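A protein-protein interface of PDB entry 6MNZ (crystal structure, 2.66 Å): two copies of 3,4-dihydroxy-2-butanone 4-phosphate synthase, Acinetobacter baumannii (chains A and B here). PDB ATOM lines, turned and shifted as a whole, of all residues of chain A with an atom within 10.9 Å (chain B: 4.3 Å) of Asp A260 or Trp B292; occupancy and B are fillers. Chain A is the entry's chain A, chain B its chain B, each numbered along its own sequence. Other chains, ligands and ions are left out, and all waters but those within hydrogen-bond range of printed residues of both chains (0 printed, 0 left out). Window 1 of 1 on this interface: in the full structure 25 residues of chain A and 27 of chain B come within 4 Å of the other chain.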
ATOM      1  N   TYR A 218     -17.946  22.955 -39.202  1.00  0.00           N
ATOM      2  CA  TYR A 218     -18.890  23.996 -39.588  1.00  0.00           C
ATOM      3  C   TYR A 218     -18.190  25.203 -40.195  1.00  0.00           C
ATOM      4  O   TYR A 218     -18.803  25.943 -40.972  1.00  0.00           O
ATOM      5  CB  TYR A 218     -19.719  24.440 -38.381  1.00  0.00           C
ATOM      6  CG  TYR A 218     -20.139  23.311 -37.469  1.00  0.00           C
ATOM      7  CD1 TYR A 218     -19.512  23.118 -36.247  1.00  0.00           C
ATOM      8  CD2 TYR A 218     -21.267  22.552 -37.749  1.00  0.00           C
ATOM      9  CE1 TYR A 218     -19.903  22.105 -35.396  1.00  0.00           C
ATOM     10  CE2 TYR A 218     -21.673  21.539 -36.900  1.00  0.00           C
ATOM     11  CZ  TYR A 218     -21.000  21.337 -35.711  1.00  0.00           C
ATOM     12  OH  TYR A 218     -21.356  20.300 -34.882  1.00  0.00           O
ATOM     13  N   HIS A 253     -25.882  27.650 -23.953  1.00  0.00           N
ATOM     14  CA  HIS A 253     -25.852  26.200 -24.112  1.00  0.00           C
ATOM     15  C   HIS A 253     -25.328  25.558 -22.836  1.00  0.00           C
ATOM     16  O   HIS A 253     -24.186  25.807 -22.438  1.00  0.00           O
ATOM     17  CB  HIS A 253     -24.983  25.795 -25.302  1.00  0.00           C
ATOM     18  CG  HIS A 253     -25.336  24.460 -25.871  1.00  0.00           C
ATOM     19  ND1 HIS A 253     -26.611  24.162 -26.300  1.00  0.00           N
ATOM     20  CD2 HIS A 253     -24.664  23.285 -25.850  1.00  0.00           C
ATOM     21  CE1 HIS A 253     -26.687  22.876 -26.587  1.00  0.00           C
ATOM     22  NE2 HIS A 253     -25.503  22.336 -26.379  1.00  0.00           N
ATOM     23  N   GLY A 254     -26.148  24.714 -22.220  1.00  0.00           N
ATOM     24  CA  GLY A 254     -25.706  23.800 -21.171  1.00  0.00           C
ATOM     25  C   GLY A 254     -25.802  22.350 -21.618  1.00  0.00           C
ATOM     26  O   GLY A 254     -26.799  21.944 -22.219  1.00  0.00           O
ATOM     27  N   PHE A 255     -24.779  21.568 -21.271  1.00  0.00           N
ATOM     28  CA  PHE A 255     -24.697  20.180 -21.714  1.00  0.00           C
ATOM     29  C   PHE A 255     -25.908  19.385 -21.237  1.00  0.00           C
ATOM     30  O   PHE A 255     -26.531  19.702 -20.221  1.00  0.00           O
ATOM     31  CB  PHE A 255     -23.413  19.540 -21.182  1.00  0.00           C
ATOM     32  CG  PHE A 255     -23.141  18.173 -21.737  1.00  0.00           C
ATOM     33  CD1 PHE A 255     -22.889  17.109 -20.885  1.00  0.00           C
ATOM     34  CD2 PHE A 255     -22.928  17.997 -23.092  1.00  0.00           C
ATOM     35  CE1 PHE A 255     -22.546  15.869 -21.387  1.00  0.00           C
ATOM     36  CE2 PHE A 255     -22.624  16.753 -23.602  1.00  0.00           C
ATOM     37  CZ  PHE A 255     -22.467  15.679 -22.749  1.00  0.00           C
ATOM     38  N   SER A 256     -26.265  18.359 -22.010  1.00  0.00           N
ATOM     39  CA  SER A 256     -27.371  17.473 -21.659  1.00  0.00           C
ATOM     40  C   SER A 256     -27.350  16.247 -22.567  1.00  0.00           C
ATOM     41  O   SER A 256     -26.490  16.153 -23.450  1.00  0.00           O
ATOM     42  CB  SER A 256     -28.701  18.219 -21.763  1.00  0.00           C
ATOM     43  OG  SER A 256     -29.346  17.941 -22.992  1.00  0.00           O
ATOM     44  N   PRO A 257     -28.219  15.252 -22.338  1.00  0.00           N
ATOM     45  CA  PRO A 257     -28.086  13.988 -23.085  1.00  0.00           C
ATOM     46  C   PRO A 257     -28.280  14.116 -24.591  1.00  0.00           C
ATOM     47  O   PRO A 257     -28.198  13.094 -25.285  1.00  0.00           O
ATOM     48  CB  PRO A 257     -29.173  13.085 -22.473  1.00  0.00           C
ATOM     49  CG  PRO A 257     -29.931  13.922 -21.493  1.00  0.00           C
ATOM     50  CD  PRO A 257     -29.091  15.111 -21.159  1.00  0.00           C
ATOM     51  N   VAL A 258     -28.663  15.286 -25.104  1.00  0.00           N
ATOM     52  CA  VAL A 258     -29.168  15.379 -26.471  1.00  0.00           C
ATOM     53  C   VAL A 258     -28.053  15.821 -27.408  1.00  0.00           C
ATOM     54  O   VAL A 258     -28.319  16.324 -28.507  1.00  0.00           O
ATOM     55  CB  VAL A 258     -30.371  16.337 -26.570  1.00  0.00           C
ATOM     56  CG1 VAL A 258     -31.501  15.852 -25.682  1.00  0.00           C
ATOM     57  CG2 VAL A 258     -29.968  17.762 -26.213  1.00  0.00           C
ATOM     58  N   ARG A 259     -26.806  15.522 -27.047  1.00  0.00           N
ATOM     59  CA  ARG A 259     -25.685  15.764 -27.945  1.00  0.00           C
ATOM     60  C   ARG A 259     -25.218  14.497 -28.644  1.00  0.00           C
ATOM     61  O   ARG A 259     -24.847  14.542 -29.821  1.00  0.00           O
ATOM     62  CB  ARG A 259     -24.500  16.357 -27.172  1.00  0.00           C
ATOM     63  CG  ARG A 259     -24.869  17.400 -26.155  1.00  0.00           C
ATOM     64  CD  ARG A 259     -25.626  18.530 -26.803  1.00  0.00           C
ATOM     65  NE  ARG A 259     -25.792  19.641 -25.880  1.00  0.00           N
ATOM     66  CZ  ARG A 259     -26.656  19.642 -24.872  1.00  0.00           C
ATOM     67  NH1 ARG A 259     -27.365  18.552 -24.609  1.00  0.00           N
ATOM     68  NH2 ARG A 259     -26.754  20.700 -24.081  1.00  0.00           N
ATOM     69  N   ASP A 260     -24.986  13.439 -27.876  1.00  0.00           N
ATOM     70  CA  ASP A 260     -24.463  12.213 -28.460  1.00  0.00           C
ATOM     71  C   ASP A 260     -25.536  11.430 -29.208  1.00  0.00           C
ATOM     72  O   ASP A 260     -25.233  10.766 -30.205  1.00  0.00           O
ATOM     73  CB  ASP A 260     -23.807  11.375 -27.368  1.00  0.00           C
ATOM     74  CG  ASP A 260     -22.645  12.101 -26.706  1.00  0.00           C
ATOM     75  OD1 ASP A 260     -22.897  12.803 -25.702  1.00  0.00           O
ATOM     76  OD2 ASP A 260     -21.615  12.281 -27.392  1.00  0.00           O
ATOM     77  N   LEU A 261     -26.777  11.438 -28.714  1.00  0.00           N
ATOM     78  CA  LEU A 261     -27.815  10.555 -29.243  1.00  0.00           C
ATOM     79  C   LEU A 261     -28.779  11.274 -30.180  1.00  0.00           C
ATOM     80  O   LEU A 261     -28.799  10.996 -31.383  1.00  0.00           O
ATOM     81  CB  LEU A 261     -28.595   9.913 -28.088  1.00  0.00           C
ATOM     82  CG  LEU A 261     -28.047   8.581 -27.579  1.00  0.00           C
ATOM     83  CD1 LEU A 261     -26.650   8.766 -27.010  1.00  0.00           C
ATOM     84  CD2 LEU A 261     -28.974   7.967 -26.539  1.00  0.00           C
ATOM     85  N   LEU A 262     -29.509  12.261 -29.670  1.00  0.00           N
ATOM     86  CA  LEU A 262     -30.225  13.200 -30.524  1.00  0.00           C
ATOM     87  C   LEU A 262     -29.257  14.314 -30.933  1.00  0.00           C
ATOM     88  O   LEU A 262     -28.039  14.200 -30.768  1.00  0.00           O
ATOM     89  CB  LEU A 262     -31.467  13.738 -29.812  1.00  0.00           C
ATOM     90  CG  LEU A 262     -32.646  12.804 -29.503  1.00  0.00           C
ATOM     91  CD1 LEU A 262     -33.684  13.569 -28.660  1.00  0.00           C
ATOM     92  CD2 LEU A 262     -33.311  12.249 -30.766  1.00  0.00           C
ATOM     93  N   LYS A 263     -29.785  15.395 -31.511  1.00  0.00           N
ATOM     94  CA  LYS A 263     -28.946  16.391 -32.179  1.00  0.00           C
ATOM     95  C   LYS A 263     -29.594  17.758 -31.969  1.00  0.00           C
ATOM     96  O   LYS A 263     -30.495  18.141 -32.722  1.00  0.00           O
ATOM     97  CB  LYS A 263     -28.784  16.073 -33.660  1.00  0.00           C
ATOM     98  CG  LYS A 263     -28.032  14.781 -33.953  1.00  0.00           C
ATOM     99  CD  LYS A 263     -27.736  14.629 -35.445  1.00  0.00           C
ATOM    100  CE  LYS A 263     -29.004  14.730 -36.288  1.00  0.00           C
ATOM    101  NZ  LYS A 263     -28.888  14.021 -37.596  1.00  0.00           N
ATOM    102  N   LEU A 264     -29.123  18.486 -30.958  1.00  0.00           N
ATOM    103  CA  LEU A 264     -29.437  19.901 -30.792  1.00  0.00           C
ATOM    104  C   LEU A 264     -28.214  20.795 -30.936  1.00  0.00           C
ATOM    105  O   LEU A 264     -28.247  21.766 -31.698  1.00  0.00           O
ATOM    106  CB  LEU A 264     -30.095  20.131 -29.422  1.00  0.00           C
ATOM    107  CG  LEU A 264     -31.224  21.165 -29.336  1.00  0.00           C
ATOM    108  CD1 LEU A 264     -32.372  20.835 -30.280  1.00  0.00           C
ATOM    109  CD2 LEU A 264     -31.734  21.271 -27.900  1.00  0.00           C
ATOM    110  N   ASN A 265     -27.137  20.514 -30.197  1.00  0.00           N
ATOM    111  CA  ASN A 265     -25.963  21.380 -30.244  1.00  0.00           C
ATOM    112  C   ASN A 265     -25.379  21.454 -31.651  1.00  0.00           C
ATOM    113  O   ASN A 265     -24.887  22.509 -32.067  1.00  0.00           O
ATOM    114  CB  ASN A 265     -24.903  20.887 -29.259  1.00  0.00           C
ATOM    115  CG  ASN A 265     -23.693  21.800 -29.201  1.00  0.00           C
ATOM    116  OD1 ASN A 265     -23.815  23.017 -29.331  1.00  0.00           O
ATOM    117  ND2 ASN A 265     -22.522  21.218 -28.969  1.00  0.00           N
ATOM    118  N   LYS A 266     -25.265  20.308 -32.327  1.00  0.00           N
ATOM    119  CA  LYS A 266     -24.821  20.316 -33.717  1.00  0.00           C
ATOM    120  C   LYS A 266     -25.762  21.143 -34.583  1.00  0.00           C
ATOM    121  O   LYS A 266     -25.353  22.155 -35.163  1.00  0.00           O
ATOM    122  CB  LYS A 266     -24.721  18.887 -34.250  1.00  0.00           C
ATOM    123  CG  LYS A 266     -23.892  18.772 -35.519  1.00  0.00           C
ATOM    124  CD  LYS A 266     -24.757  18.595 -36.757  1.00  0.00           C
ATOM    125  CE  LYS A 266     -23.919  18.712 -38.024  1.00  0.00           C
ATOM    126  NZ  LYS A 266     -24.681  18.352 -39.251  1.00  0.00           N
ATOM    127  N   ALA A 267     -27.062  20.869 -34.483  1.00  0.00           N
ATOM    128  CA  ALA A 267     -28.074  21.653 -35.179  1.00  0.00           C
ATOM    129  C   ALA A 267     -28.118  23.086 -34.664  1.00  0.00           C
ATOM    130  O   ALA A 267     -29.022  23.848 -35.021  1.00  0.00           O
ATOM    131  CB  ALA A 267     -29.450  21.001 -35.028  1.00  0.00           C
ATOM    132  N   TRP A 292     -21.224  28.830 -23.940  1.00  0.00           N
ATOM    133  CA  TRP A 292     -21.052  27.544 -23.277  1.00  0.00           C
ATOM    134  C   TRP A 292     -20.744  27.806 -21.812  1.00  0.00           C
ATOM    135  O   TRP A 292     -19.763  28.487 -21.498  1.00  0.00           O
ATOM    136  CB  TRP A 292     -19.929  26.727 -23.923  1.00  0.00           C
ATOM    137  CG  TRP A 292     -19.687  25.406 -23.253  1.00  0.00           C
ATOM    138  CD1 TRP A 292     -18.873  25.169 -22.185  1.00  0.00           C
ATOM    139  CD2 TRP A 292     -20.160  24.124 -23.687  1.00  0.00           C
ATOM    140  NE1 TRP A 292     -18.846  23.826 -21.900  1.00  0.00           N
ATOM    141  CE2 TRP A 292     -19.619  23.161 -22.814  1.00  0.00           C
ATOM    142  CE3 TRP A 292     -21.034  23.705 -24.695  1.00  0.00           C
ATOM    143  CZ2 TRP A 292     -19.995  21.819 -22.859  1.00  0.00           C
ATOM    144  CZ3 TRP A 292     -21.364  22.362 -24.771  1.00  0.00           C
ATOM    145  CH2 TRP A 292     -20.874  21.443 -23.837  1.00  0.00           C
ATOM    146  N   LEU A 298     -19.253  17.396 -16.291  1.00  0.00           N
ATOM    147  CA  LEU A 298     -20.358  17.139 -17.204  1.00  0.00           C
ATOM    148  C   LEU A 298     -20.906  15.741 -16.948  1.00  0.00           C
ATOM    149  O   LEU A 298     -20.149  14.764 -16.942  1.00  0.00           O
ATOM    150  CB  LEU A 298     -19.909  17.273 -18.658  1.00  0.00           C
ATOM    151  CG  LEU A 298     -19.560  18.684 -19.138  1.00  0.00           C
ATOM    152  CD1 LEU A 298     -19.163  18.663 -20.608  1.00  0.00           C
ATOM    153  CD2 LEU A 298     -20.723  19.639 -18.911  1.00  0.00           C
ATOM    154  N   GLN A 299     -22.214  15.655 -16.717  1.00  0.00           N
ATOM    155  CA  GLN A 299     -22.833  14.373 -16.418  1.00  0.00           C
ATOM    156  C   GLN A 299     -22.527  13.375 -17.524  1.00  0.00           C
ATOM    157  O   GLN A 299     -22.574  13.704 -18.712  1.00  0.00           O
ATOM    158  CB  GLN A 299     -24.345  14.531 -16.259  1.00  0.00           C
ATOM    159  CG  GLN A 299     -25.055  13.242 -15.868  1.00  0.00           C
ATOM    160  CD  GLN A 299     -26.544  13.428 -15.657  1.00  0.00           C
ATOM    161  OE1 GLN A 299     -27.159  14.300 -16.269  1.00  0.00           O
ATOM    162  NE2 GLN A 299     -27.154  12.498 -14.933  1.00  0.00           N
ATOM    163  N   ASP A 300     -22.292  12.129 -17.132  1.00  0.00           N
ATOM    164  CA  ASP A 300     -22.056  11.077 -18.104  1.00  0.00           C
ATOM    165  C   ASP A 300     -23.372  10.625 -18.727  1.00  0.00           C
ATOM    166  O   ASP A 300     -24.463  10.947 -18.247  1.00  0.00           O
ATOM    167  CB  ASP A 300     -21.343   9.896 -17.444  1.00  0.00           C
ATOM    168  CG  ASP A 300     -20.801   8.907 -18.453  1.00  0.00           C
ATOM    169  OD1 ASP A 300     -20.722   7.706 -18.119  1.00  0.00           O
ATOM    170  OD2 ASP A 300     -20.569   9.308 -19.612  1.00  0.00           O
ATOM    171  N   LEU A 301     -23.259   9.941 -19.867  1.00  0.00           N
ATOM    172  CA  LEU A 301     -24.447   9.616 -20.646  1.00  0.00           C
ATOM    173  C   LEU A 301     -25.292   8.547 -19.964  1.00  0.00           C
ATOM    174  O   LEU A 301     -26.519   8.546 -20.109  1.00  0.00           O
ATOM    175  CB  LEU A 301     -24.042   9.160 -22.047  1.00  0.00           C
ATOM    176  CG  LEU A 301     -25.181   8.715 -22.966  1.00  0.00           C
ATOM    177  CD1 LEU A 301     -26.255   9.788 -23.072  1.00  0.00           C
ATOM    178  CD2 LEU A 301     -24.635   8.362 -24.339  1.00  0.00           C
ATOM    179  N   GLY A 302     -24.664   7.651 -19.208  1.00  0.00           N
ATOM    180  CA  GLY A 302     -25.362   6.553 -18.585  1.00  0.00           C
ATOM    181  C   GLY A 302     -26.283   7.006 -17.472  1.00  0.00           C
ATOM    182  O   GLY A 302     -27.474   6.679 -17.453  1.00  0.00           O
ATOM    183  N   PRO A 303     -25.730   7.720 -16.481  1.00  0.00           N
ATOM    184  CA  PRO A 303     -26.476   7.959 -15.237  1.00  0.00           C
ATOM    185  C   PRO A 303     -27.871   8.513 -15.474  1.00  0.00           C
ATOM    186  O   PRO A 303     -28.029   9.542 -16.139  1.00  0.00           O
ATOM    187  CB  PRO A 303     -25.591   8.968 -14.494  1.00  0.00           C
ATOM    188  CG  PRO A 303     -24.206   8.635 -14.941  1.00  0.00           C
ATOM    189  CD  PRO A 303     -24.316   8.122 -16.362  1.00  0.00           C
ATOM    190  N   LEU A 305     -29.909   7.879 -17.663  1.00  0.00           N
ATOM    191  CA  LEU A 305     -30.216   8.200 -19.052  1.00  0.00           C
ATOM    192  C   LEU A 305     -29.762   7.080 -19.980  1.00  0.00           C
ATOM    193  O   LEU A 305     -29.585   7.294 -21.179  1.00  0.00           O
ATOM    194  CB  LEU A 305     -29.544   9.508 -19.467  1.00  0.00           C
ATOM    195  CG  LEU A 305     -29.886  10.756 -18.657  1.00  0.00           C
ATOM    196  CD1 LEU A 305     -28.838  11.831 -18.902  1.00  0.00           C
ATOM    197  CD2 LEU A 305     -31.277  11.259 -19.007  1.00  0.00           C
ATOM    198  N   TYR B 218     -30.599   9.237 -35.915  1.00  0.00           N
ATOM    199  CA  TYR B 218     -30.020   8.255 -36.823  1.00  0.00           C
ATOM    200  C   TYR B 218     -30.946   7.067 -37.043  1.00  0.00           C
ATOM    201  O   TYR B 218     -30.839   6.385 -38.069  1.00  0.00           O
ATOM    202  CB  TYR B 218     -28.675   7.761 -36.289  1.00  0.00           C
ATOM    203  CG  TYR B 218     -27.897   8.800 -35.520  1.00  0.00           C
ATOM    204  CD1 TYR B 218     -27.824   8.752 -34.135  1.00  0.00           C
ATOM    205  CD2 TYR B 218     -27.114   9.735 -36.182  1.00  0.00           C
ATOM    206  CE1 TYR B 218     -27.093   9.682 -33.428  1.00  0.00           C
ATOM    207  CE2 TYR B 218     -26.380  10.671 -35.485  1.00  0.00           C
ATOM    208  CZ  TYR B 218     -26.396  10.657 -34.107  1.00  0.00           C
ATOM    209  OH  TYR B 218     -25.686  11.602 -33.405  1.00  0.00           O
ATOM    210  N   HIS B 235     -21.639   1.653 -18.551  1.00  0.00           N
ATOM    211  CA  HIS B 235     -21.185   1.525 -19.925  1.00  0.00           C
ATOM    212  C   HIS B 235     -22.352   1.131 -20.820  1.00  0.00           C
ATOM    213  O   HIS B 235     -23.237   0.370 -20.420  1.00  0.00           O
ATOM    214  CB  HIS B 235     -20.069   0.485 -20.031  1.00  0.00           C
ATOM    215  CG  HIS B 235     -19.042   0.592 -18.947  1.00  0.00           C
ATOM    216  ND1 HIS B 235     -17.905   1.361 -19.075  1.00  0.00           N
ATOM    217  CD2 HIS B 235     -19.026   0.107 -17.683  1.00  0.00           C
ATOM    218  CE1 HIS B 235     -17.264   1.389 -17.920  1.00  0.00           C
ATOM    219  NE2 HIS B 235     -17.883   0.576 -17.084  1.00  0.00           N
ATOM    220  N   LEU B 236     -22.331   1.639 -22.049  1.00  0.00           N
ATOM    221  CA  LEU B 236     -23.449   1.505 -22.966  1.00  0.00           C
ATOM    222  C   LEU B 236     -23.003   0.764 -24.219  1.00  0.00           C
ATOM    223  O   LEU B 236     -21.809   0.641 -24.508  1.00  0.00           O
ATOM    224  CB  LEU B 236     -24.028   2.873 -23.348  1.00  0.00           C
ATOM    225  CG  LEU B 236     -24.501   3.739 -22.181  1.00  0.00           C
ATOM    226  CD1 LEU B 236     -24.848   5.138 -22.665  1.00  0.00           C
ATOM    227  CD2 LEU B 236     -25.693   3.097 -21.485  1.00  0.00           C
ATOM    228  N   HIS B 253     -15.653   3.671 -27.711  1.00  0.00           N
ATOM    229  CA  HIS B 253     -15.782   5.122 -27.753  1.00  0.00           C
ATOM    230  C   HIS B 253     -15.546   5.674 -26.358  1.00  0.00           C
ATOM    231  O   HIS B 253     -16.395   5.507 -25.476  1.00  0.00           O
ATOM    232  CB  HIS B 253     -17.162   5.535 -28.268  1.00  0.00           C
ATOM    233  CG  HIS B 253     -17.183   6.883 -28.913  1.00  0.00           C
ATOM    234  ND1 HIS B 253     -16.326   7.233 -29.936  1.00  0.00           N
ATOM    235  CD2 HIS B 253     -17.962   7.966 -28.689  1.00  0.00           C
ATOM    236  CE1 HIS B 253     -16.624   8.450 -30.357  1.00  0.00           C
ATOM    237  NE2 HIS B 253     -17.653   8.889 -29.657  1.00  0.00           N
ATOM    238  N   PHE B 255     -15.175   9.461 -24.414  1.00  0.00           N
ATOM    239  CA  PHE B 255     -15.519  10.857 -24.641  1.00  0.00           C
ATOM    240  C   PHE B 255     -14.265  11.701 -24.835  1.00  0.00           C
ATOM    241  O   PHE B 255     -13.142  11.267 -24.554  1.00  0.00           O
ATOM    242  CB  PHE B 255     -16.339  11.410 -23.475  1.00  0.00           C
ATOM    243  CG  PHE B 255     -16.936  12.766 -23.746  1.00  0.00           C
ATOM    244  CD1 PHE B 255     -17.776  12.962 -24.830  1.00  0.00           C
ATOM    245  CD2 PHE B 255     -16.527  13.874 -23.023  1.00  0.00           C
ATOM    246  CE1 PHE B 255     -18.331  14.205 -25.076  1.00  0.00           C
ATOM    247  CE2 PHE B 255     -17.105  15.110 -23.237  1.00  0.00           C
ATOM    248  CZ  PHE B 255     -17.996  15.280 -24.278  1.00  0.00           C
ATOM    249  N   ASN B 265     -17.889  11.376 -33.006  1.00  0.00           N
ATOM    250  CA  ASN B 265     -19.008  10.569 -32.529  1.00  0.00           C
ATOM    251  C   ASN B 265     -20.218  10.709 -33.442  1.00  0.00           C
ATOM    252  O   ASN B 265     -20.950   9.737 -33.668  1.00  0.00           O
ATOM    253  CB  ASN B 265     -19.382  10.964 -31.100  1.00  0.00           C
ATOM    254  CG  ASN B 265     -20.369   9.996 -30.467  1.00  0.00           C
ATOM    255  OD1 ASN B 265     -20.388   8.811 -30.801  1.00  0.00           O
ATOM    256  ND2 ASN B 265     -21.097  10.466 -29.459  1.00  0.00           N
ATOM    257  N   LEU B 290     -21.845   0.630 -31.202  1.00  0.00           N
ATOM    258  CA  LEU B 290     -21.093   1.674 -30.517  1.00  0.00           C
ATOM    259  C   LEU B 290     -21.043   1.353 -29.028  1.00  0.00           C
ATOM    260  O   LEU B 290     -22.085   1.302 -28.368  1.00  0.00           O
ATOM    261  CB  LEU B 290     -21.726   3.045 -30.750  1.00  0.00           C
ATOM    262  CG  LEU B 290     -20.975   4.234 -30.148  1.00  0.00           C
ATOM    263  CD1 LEU B 290     -21.013   5.430 -31.088  1.00  0.00           C
ATOM    264  CD2 LEU B 290     -21.548   4.606 -28.787  1.00  0.00           C
ATOM    265  N   VAL B 291     -19.835   1.243 -28.489  1.00  0.00           N
ATOM    266  CA  VAL B 291     -19.642   1.150 -27.050  1.00  0.00           C
ATOM    267  C   VAL B 291     -19.403   2.545 -26.485  1.00  0.00           C
ATOM    268  O   VAL B 291     -19.138   3.501 -27.216  1.00  0.00           O
ATOM    269  CB  VAL B 291     -18.476   0.204 -26.699  1.00  0.00           C
ATOM    270  CG1 VAL B 291     -18.535  -0.189 -25.232  1.00  0.00           C
ATOM    271  CG2 VAL B 291     -18.501  -1.030 -27.593  1.00  0.00           C
ATOM    272  N   TRP B 292     -19.682   2.694 -25.191  1.00  0.00           N
ATOM    273  CA  TRP B 292     -19.423   3.935 -24.470  1.00  0.00           C
ATOM    274  C   TRP B 292     -18.941   3.589 -23.072  1.00  0.00           C
ATOM    275  O   TRP B 292     -19.591   2.811 -22.368  1.00  0.00           O
ATOM    276  CB  TRP B 292     -20.681   4.806 -24.405  1.00  0.00           C
ATOM    277  CG  TRP B 292     -20.476   6.116 -23.707  1.00  0.00           C
ATOM    278  CD1 TRP B 292     -20.607   6.356 -22.371  1.00  0.00           C
ATOM    279  CD2 TRP B 292     -20.311   7.396 -24.330  1.00  0.00           C
ATOM    280  NE1 TRP B 292     -20.472   7.699 -22.116  1.00  0.00           N
ATOM    281  CE2 TRP B 292     -20.286   8.360 -23.302  1.00  0.00           C
ATOM    282  CE3 TRP B 292     -20.094   7.810 -25.647  1.00  0.00           C
ATOM    283  CZ2 TRP B 292     -20.009   9.703 -23.546  1.00  0.00           C
ATOM    284  CZ3 TRP B 292     -19.870   9.152 -25.892  1.00  0.00           C
ATOM    285  CH2 TRP B 292     -19.806  10.079 -24.846  1.00  0.00           C
ATOM    286  N   ILE B 293     -17.744   4.053 -22.724  1.00  0.00           N
ATOM    287  CA  ILE B 293     -17.197   3.824 -21.391  1.00  0.00           C
ATOM    288  C   ILE B 293     -17.775   4.860 -20.437  1.00  0.00           C
ATOM    289  O   ILE B 293     -17.689   6.069 -20.687  1.00  0.00           O
ATOM    290  CB  ILE B 293     -15.661   3.887 -21.413  1.00  0.00           C
ATOM    291  CG1 ILE B 293     -15.095   3.079 -22.583  1.00  0.00           C
ATOM    292  CG2 ILE B 293     -15.088   3.372 -20.101  1.00  0.00           C
ATOM    293  CD1 ILE B 293     -14.318   3.917 -23.579  1.00  0.00           C
ATOM    294  N   GLY B 294     -18.346   4.393 -19.331  1.00  0.00           N
ATOM    295  CA  GLY B 294     -18.658   5.287 -18.229  1.00  0.00           C
ATOM    296  C   GLY B 294     -17.402   5.754 -17.514  1.00  0.00           C
ATOM    297  O   GLY B 294     -16.441   5.001 -17.347  1.00  0.00           O
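5 positions are printed for both chains.
OD2 of Asp A300 is in hydrogen-bond range of NE1 of Trp B292.
The side-chain amide nitrogen of Asn B265 sits at hydrogen-bond distance from the side-chain carboxylate of Asp A260.
The backbone carbonyl oxygen (O) of Asp A260 is in hydrogen-bond range of the side-chain hydroxyl (OH) of Tyr B218 (3.3 Å).
Asp A260 touches three residues of chain B.
Of the printed residues of chain A, Trp B292 touches Asp A260 (3.8 Å), Asp A300 (3.0 Å) and Leu A301 (3.9 Å).
No residue of chain A comes within 4 Å of His B235.
Of chain A, only Leu A301 comes within 4 Å of Leu B236.
No residue of chain A comes within 4 Å of His B253.
No residue of chain A comes within 4 Å of Phe B255.
No residue of chain A comes within 4 Å of Leu B290.
No residue of chain A comes within 4 Å of Ile B293.
Gly B294 touches one residue of chain A.
Printed residues of chain B within 4 Å of Leu A261: Tyr B218 (3.0 Å).
Of the printed residues of chain A, Tyr B218 touches Asp A260 (3.3 Å), Leu A261 (3.0 Å) and Lys A263 (3.99 Å).
Printed residues of chain B within 4 Å of Leu A301: Leu B236 and Trp B292.
Asn A265 touches none of the printed residues of chain B.
Ala A267 touches none of the printed residues of chain B.
Asp A260 touches Trp B292.
Leu A261 touches Tyr B218.
Tyr B218 touches Lys A263 (OH to CG, 3.99 Å).
Asp A300 touches Gly B294 (OD1 to CA, 3.2 Å).
CD1 of Leu B236 touches CG of Leu A301, 3.6 Å away.
Trp B292 touches Leu A301.
The backbone carbonyl oxygen (O) of Val A258 sits at hydrogen-bond distance from the backbone NH (N) of Lys A263 (3.5 Å).
A ring nitrogen (ND1) of His B235 is in hydrogen-bond range of the backbone NH (N) of Gly B294, 3.1 Å away.
O of Trp B292 sits at hydrogen-bond distance from N of Leu B236 (3.0 Å).
A ring nitrogen (NE2) of His B253 sits at hydrogen-bond distance from the side-chain amide oxygen of Asn B265, 3.0 Å away.
Of the 11 printed residues of chain B, 5 touch a printed residue of chain A.
Hydrophobic or aromatic side chains of chain B that line the printed part of chain A: Tyr B218, Leu B236 and Trp B292.
Among the printed residues, 9 pairs touch across the chains.
Among the printed residues, no Asp or Glu carboxylate lies within 4 Å of a Lys or Arg side-chain nitrogen of the other chain.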
